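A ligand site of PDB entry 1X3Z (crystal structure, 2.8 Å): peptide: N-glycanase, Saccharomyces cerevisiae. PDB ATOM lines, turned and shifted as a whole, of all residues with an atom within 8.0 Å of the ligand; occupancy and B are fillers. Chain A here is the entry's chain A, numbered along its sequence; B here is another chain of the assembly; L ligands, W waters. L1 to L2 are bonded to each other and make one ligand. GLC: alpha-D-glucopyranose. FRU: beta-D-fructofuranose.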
ATOM      1  N   LYS A 110     -25.497 -13.582  35.997  1.00  0.00           N
ATOM      2  CA  LYS A 110     -24.129 -13.379  35.545  1.00  0.00           C
ATOM      3  C   LYS A 110     -23.174 -12.988  36.676  1.00  0.00           C
ATOM      4  O   LYS A 110     -22.094 -13.553  36.791  1.00  0.00           O
ATOM      5  CB  LYS A 110     -24.089 -12.369  34.400  1.00  0.00           C
ATOM      6  CG  LYS A 110     -22.711 -11.752  34.154  1.00  0.00           C
ATOM      7  CD  LYS A 110     -22.006 -12.367  32.972  1.00  0.00           C
ATOM      8  CE  LYS A 110     -20.669 -11.668  32.788  1.00  0.00           C
ATOM      9  NZ  LYS A 110     -20.358 -11.344  31.349  1.00  0.00           N
ATOM     10  N   TRP A 116     -18.695 -18.905  34.411  1.00  0.00           N
ATOM     11  CA  TRP A 116     -18.258 -19.313  33.078  1.00  0.00           C
ATOM     12  C   TRP A 116     -17.081 -20.266  33.183  1.00  0.00           C
ATOM     13  O   TRP A 116     -16.126 -20.010  33.920  1.00  0.00           O
ATOM     14  CB  TRP A 116     -17.849 -18.124  32.206  1.00  0.00           C
ATOM     15  CG  TRP A 116     -17.556 -18.587  30.815  1.00  0.00           C
ATOM     16  CD1 TRP A 116     -16.390 -19.122  30.366  1.00  0.00           C
ATOM     17  CD2 TRP A 116     -18.461 -18.607  29.703  1.00  0.00           C
ATOM     18  NE1 TRP A 116     -16.509 -19.469  29.047  1.00  0.00           N
ATOM     19  CE2 TRP A 116     -17.772 -19.154  28.615  1.00  0.00           C
ATOM     20  CE3 TRP A 116     -19.793 -18.215  29.531  1.00  0.00           C
ATOM     21  CZ2 TRP A 116     -18.357 -19.319  27.383  1.00  0.00           C
ATOM     22  CZ3 TRP A 116     -20.365 -18.376  28.302  1.00  0.00           C
ATOM     23  CH2 TRP A 116     -19.653 -18.918  27.238  1.00  0.00           C
ATOM     24  N   ASN A 118     -14.168 -21.972  31.128  1.00  0.00           N
ATOM     25  CA  ASN A 118     -13.346 -22.069  29.941  1.00  0.00           C
ATOM     26  C   ASN A 118     -12.639 -23.406  29.874  1.00  0.00           C
ATOM     27  O   ASN A 118     -12.905 -24.211  28.974  1.00  0.00           O
ATOM     28  CB  ASN A 118     -12.310 -20.951  29.896  1.00  0.00           C
ATOM     29  CG  ASN A 118     -11.657 -20.839  28.531  1.00  0.00           C
ATOM     30  OD1 ASN A 118     -12.345 -20.691  27.498  1.00  0.00           O
ATOM     31  ND2 ASN A 118     -10.323 -20.937  28.499  1.00  0.00           N
ATOM     32  N   ARG A 183     -20.723 -23.222  29.588  1.00  0.00           N
ATOM     33  CA  ARG A 183     -20.587 -22.329  28.475  1.00  0.00           C
ATOM     34  C   ARG A 183     -21.953 -21.918  27.976  1.00  0.00           C
ATOM     35  O   ARG A 183     -22.951 -22.150  28.646  1.00  0.00           O
ATOM     36  CB  ARG A 183     -19.770 -22.976  27.393  1.00  0.00           C
ATOM     37  CG  ARG A 183     -18.363 -23.091  27.858  1.00  0.00           C
ATOM     38  CD  ARG A 183     -17.554 -23.891  26.923  1.00  0.00           C
ATOM     39  NE  ARG A 183     -16.409 -24.468  27.614  1.00  0.00           N
ATOM     40  CZ  ARG A 183     -15.807 -25.580  27.223  1.00  0.00           C
ATOM     41  NH1 ARG A 183     -16.238 -26.234  26.140  1.00  0.00           N
ATOM     42  NH2 ARG A 183     -14.769 -26.053  27.908  1.00  0.00           N
ATOM     43  N   CYS A 184     -22.011 -21.290  26.806  1.00  0.00           N
ATOM     44  CA  CYS A 184     -23.268 -20.717  26.343  1.00  0.00           C
ATOM     45  C   CYS A 184     -24.373 -21.764  26.395  1.00  0.00           C
ATOM     46  O   CYS A 184     -25.487 -21.447  26.757  1.00  0.00           O
ATOM     47  CB  CYS A 184     -23.125 -20.168  24.934  1.00  0.00           C
ATOM     48  SG  CYS A 184     -22.932 -21.454  23.633  1.00  0.00           S
ATOM     49  N   GLY A 185     -24.040 -23.002  26.069  1.00  0.00           N
ATOM     50  CA  GLY A 185     -24.993 -24.103  26.099  1.00  0.00           C
ATOM     51  C   GLY A 185     -25.709 -24.139  27.412  1.00  0.00           C
ATOM     52  O   GLY A 185     -26.933 -23.917  27.492  1.00  0.00           O
ATOM     53  N   ASN A 207     -28.691 -20.599  16.957  1.00  0.00           N
ATOM     54  CA  ASN A 207     -27.919 -20.130  15.826  1.00  0.00           C
ATOM     55  C   ASN A 207     -27.023 -21.257  15.378  1.00  0.00           C
ATOM     56  O   ASN A 207     -26.264 -21.804  16.165  1.00  0.00           O
ATOM     57  CB  ASN A 207     -27.065 -18.921  16.195  1.00  0.00           C
ATOM     58  CG  ASN A 207     -26.131 -18.472  15.081  1.00  0.00           C
ATOM     59  OD1 ASN A 207     -25.077 -17.907  15.347  1.00  0.00           O
ATOM     60  ND2 ASN A 207     -26.525 -18.690  13.817  1.00  0.00           N
ATOM     61  N   GLU A 209     -24.363 -21.516  13.827  1.00  0.00           N
ATOM     62  CA  GLU A 209     -22.930 -21.429  14.014  1.00  0.00           C
ATOM     63  C   GLU A 209     -22.654 -21.367  15.499  1.00  0.00           C
ATOM     64  O   GLU A 209     -22.282 -20.316  16.026  1.00  0.00           O
ATOM     65  CB  GLU A 209     -22.328 -20.223  13.286  1.00  0.00           C
ATOM     66  CG  GLU A 209     -23.316 -19.361  12.480  1.00  0.00           C
ATOM     67  CD  GLU A 209     -23.942 -20.044  11.249  1.00  0.00           C
ATOM     68  OE1 GLU A 209     -24.413 -19.297  10.380  1.00  0.00           O
ATOM     69  OE2 GLU A 209     -23.975 -21.291  11.135  1.00  0.00           O
ATOM     70  N   ASP A 210     -22.897 -22.505  16.175  1.00  0.00           N
ATOM     71  CA  ASP A 210     -22.508 -22.741  17.575  1.00  0.00           C
ATOM     72  C   ASP A 210     -22.652 -21.513  18.526  1.00  0.00           C
ATOM     73  O   ASP A 210     -21.678 -21.050  19.128  1.00  0.00           O
ATOM     74  CB  ASP A 210     -21.105 -23.374  17.610  1.00  0.00           C
ATOM     75  CG  ASP A 210     -20.667 -23.809  19.028  1.00  0.00           C
ATOM     76  OD1 ASP A 210     -19.465 -24.154  19.201  1.00  0.00           O
ATOM     77  OD2 ASP A 210     -21.509 -23.802  19.958  1.00  0.00           O
ATOM     78  N   HIS A 211     -23.887 -20.999  18.627  1.00  0.00           N
ATOM     79  CA  HIS A 211     -24.282 -20.066  19.684  1.00  0.00           C
ATOM     80  C   HIS A 211     -25.771 -20.028  19.913  1.00  0.00           C
ATOM     81  O   HIS A 211     -26.544 -20.131  18.974  1.00  0.00           O
ATOM     82  CB  HIS A 211     -23.824 -18.642  19.427  1.00  0.00           C
ATOM     83  CG  HIS A 211     -23.878 -17.793  20.650  1.00  0.00           C
ATOM     84  ND1 HIS A 211     -23.205 -18.122  21.800  1.00  0.00           N
ATOM     85  CD2 HIS A 211     -24.541 -16.645  20.910  1.00  0.00           C
ATOM     86  CE1 HIS A 211     -23.444 -17.209  22.723  1.00  0.00           C
ATOM     87  NE2 HIS A 211     -24.250 -16.299  22.215  1.00  0.00           N
ATOM     88  N   VAL A 212     -26.150 -19.851  21.175  1.00  0.00           N
ATOM     89  CA  VAL A 212     -27.555 -19.886  21.545  1.00  0.00           C
ATOM     90  C   VAL A 212     -27.879 -18.802  22.563  1.00  0.00           C
ATOM     91  O   VAL A 212     -27.030 -18.368  23.326  1.00  0.00           O
ATOM     92  CB  VAL A 212     -27.963 -21.249  22.124  1.00  0.00           C
ATOM     93  CG1 VAL A 212     -27.991 -22.301  21.042  1.00  0.00           C
ATOM     94  CG2 VAL A 212     -27.017 -21.656  23.254  1.00  0.00           C
ATOM     95  N   ASP A 228     -29.502 -12.327  25.991  1.00  0.00           N
ATOM     96  CA  ASP A 228     -28.401 -13.279  26.123  1.00  0.00           C
ATOM     97  C   ASP A 228     -27.889 -13.211  27.543  1.00  0.00           C
ATOM     98  O   ASP A 228     -27.588 -12.145  28.035  1.00  0.00           O
ATOM     99  CB  ASP A 228     -27.289 -12.927  25.140  1.00  0.00           C
ATOM    100  CG  ASP A 228     -26.206 -13.997  25.070  1.00  0.00           C
ATOM    101  OD1 ASP A 228     -25.728 -14.459  26.136  1.00  0.00           O
ATOM    102  OD2 ASP A 228     -25.846 -14.380  23.943  1.00  0.00           O
ATOM    103  N   CYS A 230     -25.102 -14.767  28.776  1.00  0.00           N
ATOM    104  CA  CYS A 230     -23.633 -14.843  28.812  1.00  0.00           C
ATOM    105  C   CYS A 230     -23.072 -13.459  28.730  1.00  0.00           C
ATOM    106  O   CYS A 230     -22.524 -12.931  29.685  1.00  0.00           O
ATOM    107  CB  CYS A 230     -23.081 -15.564  27.607  1.00  0.00           C
ATOM    108  SG  CYS A 230     -23.728 -17.156  27.245  1.00  0.00           S
ATOM    109  N   GLU A 231     -23.171 -12.899  27.532  1.00  0.00           N
ATOM    110  CA  GLU A 231     -23.120 -11.478  27.402  1.00  0.00           C
ATOM    111  C   GLU A 231     -24.302 -11.110  28.283  1.00  0.00           C
ATOM    112  O   GLU A 231     -25.375 -11.715  28.166  1.00  0.00           O
ATOM    113  CB  GLU A 231     -23.385 -11.116  25.963  1.00  0.00           C
ATOM    114  CG  GLU A 231     -22.273 -10.336  25.324  1.00  0.00           C
ATOM    115  CD  GLU A 231     -20.929 -11.043  25.411  1.00  0.00           C
ATOM    116  OE1 GLU A 231     -20.798 -12.171  24.856  1.00  0.00           O
ATOM    117  OE2 GLU A 231     -20.011 -10.470  26.066  1.00  0.00           O
ATOM    118  N   ILE A 239     -25.385  -7.109  18.478  1.00  0.00           N
ATOM    119  CA  ILE A 239     -24.225  -7.700  19.157  1.00  0.00           C
ATOM    120  C   ILE A 239     -23.491  -8.729  18.311  1.00  0.00           C
ATOM    121  O   ILE A 239     -22.328  -8.518  17.964  1.00  0.00           O
ATOM    122  CB  ILE A 239     -24.677  -8.329  20.470  1.00  0.00           C
ATOM    123  CG1 ILE A 239     -24.847  -7.242  21.508  1.00  0.00           C
ATOM    124  CG2 ILE A 239     -23.673  -9.305  21.029  1.00  0.00           C
ATOM    125  CD1 ILE A 239     -23.549  -6.925  22.206  1.00  0.00           C
ATOM    126  N   TYR A 240     -24.154  -9.823  17.951  1.00  0.00           N
ATOM    127  CA  TYR A 240     -23.460 -10.903  17.261  1.00  0.00           C
ATOM    128  C   TYR A 240     -22.951 -10.424  15.905  1.00  0.00           C
ATOM    129  O   TYR A 240     -21.750 -10.347  15.683  1.00  0.00           O
ATOM    130  CB  TYR A 240     -24.315 -12.183  17.154  1.00  0.00           C
ATOM    131  CG  TYR A 240     -25.036 -12.561  18.446  1.00  0.00           C
ATOM    132  CD1 TYR A 240     -24.358 -12.589  19.669  1.00  0.00           C
ATOM    133  CD2 TYR A 240     -26.384 -12.898  18.454  1.00  0.00           C
ATOM    134  CE1 TYR A 240     -25.013 -12.918  20.858  1.00  0.00           C
ATOM    135  CE2 TYR A 240     -27.038 -13.236  19.622  1.00  0.00           C
ATOM    136  CZ  TYR A 240     -26.345 -13.249  20.828  1.00  0.00           C
ATOM    137  OH  TYR A 240     -27.001 -13.579  21.992  1.00  0.00           O
ATOM    138  N   ASN A 243     -21.039  -6.300  16.439  1.00  0.00           N
ATOM    139  CA  ASN A 243     -19.973  -6.169  17.449  1.00  0.00           C
ATOM    140  C   ASN A 243     -18.951  -7.293  17.471  1.00  0.00           C
ATOM    141  O   ASN A 243     -17.763  -7.055  17.633  1.00  0.00           O
ATOM    142  CB  ASN A 243     -20.543  -6.009  18.849  1.00  0.00           C
ATOM    143  CG  ASN A 243     -21.322  -4.739  19.008  1.00  0.00           C
ATOM    144  OD1 ASN A 243     -21.606  -4.324  20.127  1.00  0.00           O
ATOM    145  ND2 ASN A 243     -21.674  -4.098  17.895  1.00  0.00           N
ATOM    146  N   TRP A 244     -19.421  -8.518  17.345  1.00  0.00           N
ATOM    147  CA  TRP A 244     -18.544  -9.657  17.298  1.00  0.00           C
ATOM    148  C   TRP A 244     -18.105  -9.833  15.862  1.00  0.00           C
ATOM    149  O   TRP A 244     -17.164 -10.549  15.577  1.00  0.00           O
ATOM    150  CB  TRP A 244     -19.313 -10.905  17.666  1.00  0.00           C
ATOM    151  CG  TRP A 244     -19.734 -11.014  19.072  1.00  0.00           C
ATOM    152  CD1 TRP A 244     -19.728 -10.031  20.028  1.00  0.00           C
ATOM    153  CD2 TRP A 244     -20.264 -12.184  19.689  1.00  0.00           C
ATOM    154  NE1 TRP A 244     -20.218 -10.525  21.216  1.00  0.00           N
ATOM    155  CE2 TRP A 244     -20.550 -11.851  21.026  1.00  0.00           C
ATOM    156  CE3 TRP A 244     -20.514 -13.488  19.250  1.00  0.00           C
ATOM    157  CZ2 TRP A 244     -21.077 -12.781  21.932  1.00  0.00           C
ATOM    158  CZ3 TRP A 244     -21.043 -14.409  20.152  1.00  0.00           C
ATOM    159  CH2 TRP A 244     -21.315 -14.051  21.466  1.00  0.00           C
ATOM    160  N   ASN A 245     -18.837  -9.196  14.954  1.00  0.00           N
ATOM    161  CA  ASN A 245     -18.622  -9.378  13.538  1.00  0.00           C
ATOM    162  C   ASN A 245     -18.691 -10.850  13.155  1.00  0.00           C
ATOM    163  O   ASN A 245     -17.810 -11.356  12.480  1.00  0.00           O
ATOM    164  CB  ASN A 245     -17.308  -8.740  13.109  1.00  0.00           C
ATOM    165  CG  ASN A 245     -17.422  -8.062  11.770  1.00  0.00           C
ATOM    166  OD1 ASN A 245     -17.440  -6.832  11.691  1.00  0.00           O
ATOM    167  ND2 ASN A 245     -17.563  -8.859  10.710  1.00  0.00           N
ATOM    168  N   LYS A 246     -19.736 -11.528  13.594  1.00  0.00           N
ATOM    169  CA  LYS A 246     -19.816 -12.966  13.390  1.00  0.00           C
ATOM    170  C   LYS A 246     -20.603 -13.332  12.142  1.00  0.00           C
ATOM    171  O   LYS A 246     -21.687 -12.806  11.886  1.00  0.00           O
ATOM    172  CB  LYS A 246     -20.359 -13.665  14.640  1.00  0.00           C
ATOM    173  CG  LYS A 246     -20.676 -15.142  14.482  1.00  0.00           C
ATOM    174  CD  LYS A 246     -21.281 -15.718  15.769  1.00  0.00           C
ATOM    175  CE  LYS A 246     -21.713 -17.165  15.576  1.00  0.00           C
ATOM    176  NZ  LYS A 246     -21.371 -18.026  16.750  1.00  0.00           N
ATOM    177  N   ALA B   3     -23.775 -26.743  23.249  1.00  0.00           N
ATOM    178  CA  ALA B   3     -23.025 -25.669  22.548  1.00  0.00           C
ATOM    179  C   ALA B   3     -22.070 -24.853  23.421  1.00  0.00           C
ATOM    180  O   ALA B   3     -22.343 -24.624  24.595  1.00  0.00           O
ATOM    181  CB  ALA B   3     -23.982 -24.750  21.819  1.00  0.00           C
ATOM    182  N   ASP B   4     -20.977 -24.388  22.841  1.00  0.00           N
ATOM    183  CA  ASP B   4     -19.980 -23.591  23.576  1.00  0.00           C
ATOM    184  C   ASP B   4     -20.256 -22.099  23.449  1.00  0.00           C
ATOM    185  O   ASP B   4     -19.431 -21.382  22.847  1.00  0.00           O
ATOM    186  CB  ASP B   4     -18.575 -23.895  23.078  1.00  0.00           C
ATOM    187  CG  ASP B   4     -18.119 -25.278  23.467  1.00  0.00           C
ATOM    188  OD1 ASP B   4     -17.662 -26.014  22.552  1.00  0.00           O
ATOM    189  OD2 ASP B   4     -18.232 -25.631  24.652  1.00  0.00           O
ATOM    190  C1  CF0 B   5     -21.286 -21.582  23.927  1.00  0.00           C
HETATM  191  C1  GLC L   1     -16.404 -15.062  23.437  1.00  0.00           C
HETATM  192  C2  GLC L   1     -16.171 -14.296  24.737  1.00  0.00           C
HETATM  193  C3  GLC L   1     -17.150 -13.142  24.802  1.00  0.00           C
HETATM  194  C4  GLC L   1     -16.804 -12.207  23.655  1.00  0.00           C
HETATM  195  C5  GLC L   1     -16.977 -12.899  22.304  1.00  0.00           C
HETATM  196  C6  GLC L   1     -16.344 -12.034  21.214  1.00  0.00           C
HETATM  197  O2  GLC L   1     -16.432 -15.170  25.841  1.00  0.00           O
HETATM  198  O3  GLC L   1     -17.045 -12.497  26.064  1.00  0.00           O
HETATM  199  O4  GLC L   1     -17.643 -11.046  23.732  1.00  0.00           O
HETATM  200  O5  GLC L   1     -16.412 -14.222  22.265  1.00  0.00           O
HETATM  201  O6  GLC L   1     -16.018 -12.803  20.055  1.00  0.00           O
HETATM  202  C1  FRU L   2     -16.927 -17.933  24.373  1.00  0.00           C
HETATM  203  C2  FRU L   2     -17.590 -17.149  23.262  1.00  0.00           C
HETATM  204  C3  FRU L   2     -19.014 -17.637  23.068  1.00  0.00           C
HETATM  205  C4  FRU L   2     -19.207 -17.712  21.573  1.00  0.00           C
HETATM  206  C5  FRU L   2     -17.788 -17.793  20.997  1.00  0.00           C
HETATM  207  C6  FRU L   2     -17.579 -16.904  19.784  1.00  0.00           C
HETATM  208  O1  FRU L   2     -15.612 -18.334  23.981  1.00  0.00           O
HETATM  209  O2  FRU L   2     -17.649 -15.757  23.555  1.00  0.00           O
HETATM  210  O3  FRU L   2     -19.933 -16.713  23.640  1.00  0.00           O
HETATM  211  O4  FRU L   2     -19.999 -18.864  21.253  1.00  0.00           O
HETATM  212  O5  FRU L   2     -16.902 -17.364  22.025  1.00  0.00           O
HETATM  213  O6  FRU L   2     -16.575 -15.940  20.067  1.00  0.00           O
HETATM  214  O   HOH W   1     -17.565 -15.875  16.920  1.00  0.00           O
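An oxygen (O4) of FRU L2 lies within hydrogen-bond range of the backbone carbonyl oxygen of Asp 4 of chain B (3.0 Å). A ring nitrogen (ND1) of His 211 is in hydrogen-bond range of an oxygen (O4) of FRU L2 (3.3 Å). The side-chain carboxylate (OE2) of Glu 231 sits at hydrogen-bond distance from an oxygen (O4) of GLC L1 (3.4 Å). O of Asp 210 sits at hydrogen-bond distance from O4 of FRU L2.
Merely in contact with the ligand: Trp 116 (3.6 Å) and Trp 244 (3.6 Å). Within 4 Å of the ligand: Trp 116, Asp 210, His 211, Glu 231, Trp 244 and Asp 4 of chain B.
The side-chain sulfur (SG) of Cys 184 lies close to the backbone NH (N) of Asp 4 of chain B (3.6 Å). The side-chain carboxylate (OD2) of Asp 210 sits at hydrogen-bond distance from the backbone NH (N) of Asp 4 of chain B (3.0 Å). OD1 of Asp 228 sits at hydrogen-bond distance from N of Glu 231. The side-chain carboxylate (OD2) of Asp 228 sits at hydrogen-bond distance from a ring nitrogen (NE2) of His 211, 3.0 Å away. N of Trp 244 sits at hydrogen-bond distance from O of Ile 239. The side-chain carboxylate of Asp 4 of chain B is in salt-bridge range of the guanidinium group of Arg 183, at 2.6 Å.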
